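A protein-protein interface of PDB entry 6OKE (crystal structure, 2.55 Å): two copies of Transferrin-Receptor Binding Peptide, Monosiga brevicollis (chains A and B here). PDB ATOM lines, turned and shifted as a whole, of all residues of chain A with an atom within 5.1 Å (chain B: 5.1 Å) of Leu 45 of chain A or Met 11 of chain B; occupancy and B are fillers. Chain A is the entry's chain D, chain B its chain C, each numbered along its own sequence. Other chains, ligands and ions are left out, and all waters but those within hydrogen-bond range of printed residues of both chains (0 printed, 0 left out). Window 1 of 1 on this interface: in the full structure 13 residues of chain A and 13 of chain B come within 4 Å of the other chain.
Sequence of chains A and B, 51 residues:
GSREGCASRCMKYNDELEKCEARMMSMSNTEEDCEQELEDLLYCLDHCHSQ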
ATOM      1  N   ALA A   7      26.218   1.626  -0.581  1.00  0.00           N
ATOM      2  CA  ALA A   7      26.241   0.451   0.324  1.00  0.00           C
ATOM      3  C   ALA A   7      26.951  -0.723  -0.362  1.00  0.00           C
ATOM      4  O   ALA A   7      27.741  -1.414   0.316  1.00  0.00           O
ATOM      5  CB  ALA A   7      24.839   0.078   0.736  1.00  0.00           C
ATOM      6  N   CYS A  10      30.617  -0.989  -0.173  1.00  0.00           N
ATOM      7  CA  CYS A  10      31.060  -1.317   1.210  1.00  0.00           C
ATOM      8  C   CYS A  10      31.011  -2.834   1.444  1.00  0.00           C
ATOM      9  O   CYS A  10      31.517  -3.262   2.487  1.00  0.00           O
ATOM     10  CB  CYS A  10      30.195  -0.636   2.268  1.00  0.00           C
ATOM     11  SG  CYS A  10      30.182   1.184   2.228  1.00  0.00           S
ATOM     12  N   LEU A  41      34.717  -1.025   7.735  1.00  0.00           N
ATOM     13  CA  LEU A  41      33.357  -1.455   7.308  1.00  0.00           C
ATOM     14  C   LEU A  41      32.333  -0.498   7.915  1.00  0.00           C
ATOM     15  O   LEU A  41      31.439  -0.037   7.168  1.00  0.00           O
ATOM     16  CB  LEU A  41      33.107  -2.890   7.771  1.00  0.00           C
ATOM     17  CG  LEU A  41      31.690  -3.427   7.608  1.00  0.00           C
ATOM     18  CD1 LEU A  41      31.218  -3.316   6.169  1.00  0.00           C
ATOM     19  CD2 LEU A  41      31.637  -4.879   8.073  1.00  0.00           C
ATOM     20  N   LEU A  42      32.454  -0.206   9.215  1.00  0.00           N
ATOM     21  CA  LEU A  42      31.492   0.675   9.920  1.00  0.00           C
ATOM     22  C   LEU A  42      31.631   2.098   9.377  1.00  0.00           C
ATOM     23  O   LEU A  42      30.579   2.686   9.046  1.00  0.00           O
ATOM     24  CB  LEU A  42      31.725   0.577  11.429  1.00  0.00           C
ATOM     25  CG  LEU A  42      31.443  -0.800  12.028  1.00  0.00           C
ATOM     26  CD1 LEU A  42      31.370  -0.738  13.543  1.00  0.00           C
ATOM     27  CD2 LEU A  42      30.145  -1.367  11.468  1.00  0.00           C
ATOM     28  N   TYR A  43      32.864   2.596   9.236  1.00  0.00           N
ATOM     29  CA  TYR A  43      33.193   3.889   8.575  1.00  0.00           C
ATOM     30  C   TYR A  43      32.447   3.958   7.238  1.00  0.00           C
ATOM     31  O   TYR A  43      31.667   4.899   7.035  1.00  0.00           O
ATOM     32  CB  TYR A  43      34.706   4.038   8.360  1.00  0.00           C
ATOM     33  CG  TYR A  43      35.510   4.537   9.538  1.00  0.00           C
ATOM     34  CD1 TYR A  43      35.080   4.354  10.841  1.00  0.00           C
ATOM     35  CD2 TYR A  43      36.750   5.120   9.352  1.00  0.00           C
ATOM     36  CE1 TYR A  43      35.824   4.798  11.923  1.00  0.00           C
ATOM     37  CE2 TYR A  43      37.519   5.557  10.422  1.00  0.00           C
ATOM     38  CZ  TYR A  43      37.053   5.398  11.716  1.00  0.00           C
ATOM     39  OH  TYR A  43      37.774   5.817  12.796  1.00  0.00           O
ATOM     40  N   CYS A  44      32.646   2.969   6.368  1.00  0.00           N
ATOM     41  CA  CYS A  44      32.013   2.906   5.024  1.00  0.00           C
ATOM     42  C   CYS A  44      30.485   2.970   5.152  1.00  0.00           C
ATOM     43  O   CYS A  44      29.868   3.805   4.466  1.00  0.00           O
ATOM     44  CB  CYS A  44      32.414   1.645   4.277  1.00  0.00           C
ATOM     45  SG  CYS A  44      32.087   1.781   2.502  1.00  0.00           S
ATOM     46  N   LEU A  45      29.894   2.119   5.996  1.00  0.00           N
ATOM     47  CA  LEU A  45      28.419   2.060   6.198  1.00  0.00           C
ATOM     48  C   LEU A  45      27.908   3.401   6.730  1.00  0.00           C
ATOM     49  O   LEU A  45      26.786   3.784   6.391  1.00  0.00           O
ATOM     50  CB  LEU A  45      28.083   0.929   7.172  1.00  0.00           C
ATOM     51  CG  LEU A  45      28.190  -0.475   6.589  1.00  0.00           C
ATOM     52  CD1 LEU A  45      27.918  -1.512   7.664  1.00  0.00           C
ATOM     53  CD2 LEU A  45      27.235  -0.656   5.419  1.00  0.00           C
ATOM     54  N   ASP A  46      28.707   4.066   7.558  1.00  0.00           N
ATOM     55  CA  ASP A  46      28.338   5.328   8.254  1.00  0.00           C
ATOM     56  C   ASP A  46      28.179   6.433   7.212  1.00  0.00           C
ATOM     57  O   ASP A  46      27.178   7.176   7.298  1.00  0.00           O
ATOM     58  CB  ASP A  46      29.371   5.684   9.325  1.00  0.00           C
ATOM     59  CG  ASP A  46      28.998   6.903  10.130  1.00  0.00           C
ATOM     60  OD1 ASP A  46      28.965   8.000   9.545  1.00  0.00           O
ATOM     61  OD2 ASP A  46      28.739   6.732  11.342  1.00  0.00           O
ATOM     62  N   HIS A  47      29.128   6.531   6.277  1.00  0.00           N
ATOM     63  CA  HIS A  47      29.150   7.547   5.192  1.00  0.00           C
ATOM     64  C   HIS A  47      27.962   7.347   4.239  1.00  0.00           C
ATOM     65  O   HIS A  47      27.402   8.361   3.795  1.00  0.00           O
ATOM     66  CB  HIS A  47      30.498   7.500   4.467  1.00  0.00           C
ATOM     67  N   CYS A  48      27.567   6.104   3.954  1.00  0.00           N
ATOM     68  CA  CYS A  48      26.372   5.789   3.124  1.00  0.00           C
ATOM     69  C   CYS A  48      25.125   6.339   3.813  1.00  0.00           C
ATOM     70  O   CYS A  48      24.275   6.907   3.112  1.00  0.00           O
ATOM     71  CB  CYS A  48      26.162   4.294   2.916  1.00  0.00           C
ATOM     72  SG  CYS A  48      27.381   3.499   1.838  1.00  0.00           S
ATOM     73  N   HIS A  49      25.032   6.143   5.131  1.00  0.00           N
ATOM     74  CA  HIS A  49      23.893   6.562   5.995  1.00  0.00           C
ATOM     75  C   HIS A  49      23.669   8.079   5.885  1.00  0.00           C
ATOM     76  O   HIS A  49      22.490   8.487   5.771  1.00  0.00           O
ATOM     77  CB  HIS A  49      24.129   6.107   7.444  1.00  0.00           C
ATOM     78  CG  HIS A  49      23.021   6.455   8.379  1.00  0.00           C
ATOM     79  ND1 HIS A  49      22.065   5.537   8.769  1.00  0.00           N
ATOM     80  CD2 HIS A  49      22.711   7.612   9.003  1.00  0.00           C
ATOM     81  CE1 HIS A  49      21.214   6.113   9.593  1.00  0.00           C
ATOM     82  NE2 HIS A  49      21.587   7.389   9.748  1.00  0.00           N
ATOM     83  N   ALA B   7      24.537  -5.586   0.186  1.00  0.00           N
ATOM     84  CA  ALA B   7      24.922  -4.678   1.288  1.00  0.00           C
ATOM     85  C   ALA B   7      23.763  -3.731   1.606  1.00  0.00           C
ATOM     86  O   ALA B   7      23.513  -3.507   2.803  1.00  0.00           O
ATOM     87  CB  ALA B   7      26.177  -3.925   0.926  1.00  0.00           C
ATOM     88  N   SER B   8      23.089  -3.206   0.576  1.00  0.00           N
ATOM     89  CA  SER B   8      21.941  -2.272   0.707  1.00  0.00           C
ATOM     90  C   SER B   8      20.842  -2.923   1.554  1.00  0.00           C
ATOM     91  O   SER B   8      20.282  -2.221   2.411  1.00  0.00           O
ATOM     92  CB  SER B   8      21.413  -1.836  -0.640  1.00  0.00           C
ATOM     93  OG  SER B   8      20.651  -2.866  -1.251  1.00  0.00           O
ATOM     94  N   ARG B   9      20.590  -4.224   1.364  1.00  0.00           N
ATOM     95  CA  ARG B   9      19.536  -5.001   2.077  1.00  0.00           C
ATOM     96  C   ARG B   9      19.880  -5.139   3.568  1.00  0.00           C
ATOM     97  O   ARG B   9      18.988  -5.587   4.331  1.00  0.00           O
ATOM     98  CB  ARG B   9      19.355  -6.384   1.443  1.00  0.00           C
ATOM     99  N   CYS B  10      21.117  -4.789   3.970  1.00  0.00           N
ATOM    100  CA  CYS B  10      21.597  -4.849   5.380  1.00  0.00           C
ATOM    101  C   CYS B  10      21.718  -3.444   5.978  1.00  0.00           C
ATOM    102  O   CYS B  10      22.186  -3.329   7.103  1.00  0.00           O
ATOM    103  CB  CYS B  10      22.925  -5.592   5.494  1.00  0.00           C
ATOM    104  SG  CYS B  10      22.830  -7.356   5.064  1.00  0.00           S
ATOM    105  N   MET B  11      21.308  -2.411   5.249  1.00  0.00           N
ATOM    106  CA  MET B  11      21.455  -0.996   5.685  1.00  0.00           C
ATOM    107  C   MET B  11      20.501  -0.750   6.855  1.00  0.00           C
ATOM    108  O   MET B  11      20.880   0.017   7.760  1.00  0.00           O
ATOM    109  CB  MET B  11      21.162  -0.003   4.557  1.00  0.00           C
ATOM    110  CG  MET B  11      22.368   0.254   3.661  1.00  0.00           C
ATOM    111  SD  MET B  11      23.850   0.826   4.565  1.00  0.00           S
ATOM    112  CE  MET B  11      23.375   2.509   4.959  1.00  0.00           C
ATOM    113  N   LYS B  12      19.335  -1.400   6.867  1.00  0.00           N
ATOM    114  CA  LYS B  12      18.339  -1.286   7.968  1.00  0.00           C
ATOM    115  C   LYS B  12      18.992  -1.692   9.293  1.00  0.00           C
ATOM    116  O   LYS B  12      18.607  -1.141  10.340  1.00  0.00           O
ATOM    117  CB  LYS B  12      17.087  -2.113   7.664  1.00  0.00           C
ATOM    118  CG  LYS B  12      17.245  -3.620   7.685  1.00  0.00           C
ATOM    119  CD  LYS B  12      16.137  -4.313   6.921  1.00  0.00           C
ATOM    120  CE  LYS B  12      16.204  -5.818   7.031  1.00  0.00           C
ATOM    121  NZ  LYS B  12      15.994  -6.266   8.430  1.00  0.00           N
ATOM    122  N   TYR B  13      19.949  -2.617   9.250  1.00  0.00           N
ATOM    123  CA  TYR B  13      20.692  -3.118  10.439  1.00  0.00           C
ATOM    124  C   TYR B  13      21.725  -2.074  10.869  1.00  0.00           C
ATOM    125  O   TYR B  13      21.991  -1.965  12.068  1.00  0.00           O
ATOM    126  CB  TYR B  13      21.308  -4.487  10.148  1.00  0.00           C
ATOM    127  CG  TYR B  13      20.279  -5.583  10.047  1.00  0.00           C
ATOM    128  CD1 TYR B  13      19.646  -6.062  11.181  1.00  0.00           C
ATOM    129  CD2 TYR B  13      19.900  -6.106   8.822  1.00  0.00           C
ATOM    130  CE1 TYR B  13      18.714  -7.082  11.106  1.00  0.00           C
ATOM    131  CE2 TYR B  13      18.947  -7.110   8.728  1.00  0.00           C
ATOM    132  CZ  TYR B  13      18.363  -7.611   9.877  1.00  0.00           C
ATOM    133  OH  TYR B  13      17.426  -8.603   9.801  1.00  0.00           O
ATOM    134  N   ASN B  14      22.275  -1.316   9.920  1.00  0.00           N
ATOM    135  CA  ASN B  14      23.141  -0.143  10.219  1.00  0.00           C
ATOM    136  C   ASN B  14      22.282   0.952  10.854  1.00  0.00           C
ATOM    137  O   ASN B  14      22.701   1.492  11.873  1.00  0.00           O
ATOM    138  CB  ASN B  14      23.870   0.371   8.978  1.00  0.00           C
ATOM    139  CG  ASN B  14      25.019   1.289   9.323  1.00  0.00           C
ATOM    140  OD1 ASN B  14      24.993   2.473   8.988  1.00  0.00           O
ATOM    141  ND2 ASN B  14      25.998   0.757  10.031  1.00  0.00           N
ATOM    142  N   ASP B  15      21.117   1.260  10.284  1.00  0.00           N
ATOM    143  CA  ASP B  15      20.154   2.248  10.849  1.00  0.00           C
ATOM    144  C   ASP B  15      19.947   1.943  12.338  1.00  0.00           C
ATOM    145  O   ASP B  15      20.116   2.860  13.148  1.00  0.00           O
ATOM    146  CB  ASP B  15      18.809   2.243  10.113  1.00  0.00           C
ATOM    147  CG  ASP B  15      18.879   2.601   8.638  1.00  0.00           C
ATOM    148  OD1 ASP B  15      19.965   3.027   8.172  1.00  0.00           O
ATOM    149  OD2 ASP B  15      17.841   2.438   7.960  1.00  0.00           O
ATOM    150  N   GLU B  18      23.067   2.755  14.246  1.00  0.00           N
ATOM    151  CA  GLU B  18      23.164   4.239  14.315  1.00  0.00           C
ATOM    152  C   GLU B  18      22.283   4.739  15.462  1.00  0.00           C
ATOM    153  O   GLU B  18      22.791   5.506  16.288  1.00  0.00           O
ATOM    154  CB  GLU B  18      22.740   4.907  13.003  1.00  0.00           C
ATOM    155  CG  GLU B  18      23.614   4.535  11.813  1.00  0.00           C
ATOM    156  CD  GLU B  18      25.010   5.136  11.782  1.00  0.00           C
ATOM    157  OE1 GLU B  18      25.311   5.992  12.646  1.00  0.00           O
ATOM    158  OE2 GLU B  18      25.797   4.772  10.862  1.00  0.00           O
ATOM    159  N   LEU B  41      24.020  -6.925  12.251  1.00  0.00           N
ATOM    160  CA  LEU B  41      24.593  -6.303  11.025  1.00  0.00           C
ATOM    161  C   LEU B  41      25.596  -7.272  10.389  1.00  0.00           C
ATOM    162  O   LEU B  41      25.521  -7.492   9.161  1.00  0.00           O
ATOM    163  CB  LEU B  41      25.260  -4.979  11.399  1.00  0.00           C
ATOM    164  CG  LEU B  41      26.059  -4.300  10.289  1.00  0.00           C
ATOM    165  CD1 LEU B  41      25.199  -4.065   9.056  1.00  0.00           C
ATOM    166  CD2 LEU B  41      26.655  -2.992  10.783  1.00  0.00           C
ATOM    167  N   LEU B  45      25.362  -9.238   6.835  1.00  0.00           N
ATOM    168  CA  LEU B  45      26.433  -9.079   5.816  1.00  0.00           C
ATOM    169  C   LEU B  45      27.017 -10.450   5.471  1.00  0.00           C
ATOM    170  O   LEU B  45      27.370 -10.660   4.297  1.00  0.00           O
ATOM    171  CB  LEU B  45      27.510  -8.138   6.350  1.00  0.00           C
ATOM    172  CG  LEU B  45      27.110  -6.661   6.383  1.00  0.00           C
ATOM    173  CD1 LEU B  45      28.208  -5.815   6.996  1.00  0.00           C
ATOM    174  CD2 LEU B  45      26.756  -6.148   4.987  1.00  0.00           C
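Cys 10 of chain A touches none of the printed residues of chain B. Cys 44 of chain A touches none of the printed residues of chain B. Of the printed residues of chain A, Met 11 of chain B touches Ala 7, Leu 45, Cys 48 and His 49. Printed residues of chain A within 4 Å of Glu 18 of chain B: Asp 46 (3.6 Å) and His 49 (3.6 Å). Printed residues of chain A within 4 Å of Leu 45 of chain B: Leu 41 (3.7 Å). The nearest residue of chain B that does not touch Leu 45 of chain A is Leu 45 of chain B (4.4 Å). The nearest printed residue of chain A that does not touch Met 11 of chain B is Asp 46 of chain A (6.1 Å).
Of the 12 printed residues of chain B, 8 touch a printed residue of chain A. Hydrophobic or aromatic side chains of chain B within 4 Å of the printed part of chain A: Ala 7, Met 11, Leu 41 and Leu 45. Hydrophobic or aromatic side chains of chain A that line the printed part of chain B: Ala 7, Leu 41, Leu 42, Leu 45 and His 49. Along chain A the printed residues that touch a printed residue of chain B span positions 7 to 49. Among the printed residues, no Asp or Glu carboxylate lies within 4 Å of a Lys or Arg side-chain nitrogen of the other chain.
OD1 of Asn 14 of chain B sits close to O of Leu 45 of chain A (3.4 Å). The side-chain carboxylate (OD1) of Asp 15 of chain B is in hydrogen-bond range of a ring nitrogen (ND1) of His 49 of chain A, 3.3 Å away.
Among the printed residues, pairs that only touch across the chains: Ala 7 of chain A with Ala 7 of chain B (3.0 Å), Ala 7 of chain A with Ser 8 of chain B (3.7 Å), Ala 7 of chain A with Met 11 of chain B (3.8 Å), Leu 41 of chain A with Leu 45 of chain B (3.7 Å), Leu 42 of chain A with Leu 41 of chain B (3.9 Å), Leu 45 of chain A with Met 11 of chain B (3.8 Å), Leu 45 of chain A with Leu 41 of chain B (3.7 Å), Asp 46 of chain A with Glu 18 of chain B (3.6 Å), Cys 48 of chain A with Met 11 of chain B (3.9 Å), His 49 of chain A with Met 11 of chain B (3.998 Å) and His 49 of chain A with Glu 18 of chain B (3.6 Å).
The backbone NH of Leu 45 of chain B is in hydrogen-bond range of the side-chain sulfur of Cys 10 of chain B (3.6 Å). The side-chain carboxylate (OE2) of Glu 18 of chain B lies close to the side-chain amide oxygen (OD1) of Asn 14 of chain B (3.1 Å). The backbone NH of Ala 7 of chain A is in hydrogen-bond range of the side-chain sulfur of Cys 48 of chain A (3.3 Å). The side-chain sulfur (SG) of Cys 10 of chain A forms a disulfide with the side-chain sulfur (SG) of Cys 44 of chain A, at 2.0 Å.
Ala 7 of chain A touches its own counterpart, Ala 7 of chain B. Leu 41 of chain A touches Leu 45 of chain B, and with the chains exchanged Leu 45 of chain A touches Leu 41 of chain B. Positions printed for both chains: 7, 10, 41 and 45. Of the 13 pairs that touch across the chains among the printed residues, 3 have their exchanged pair printed and touching as well.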
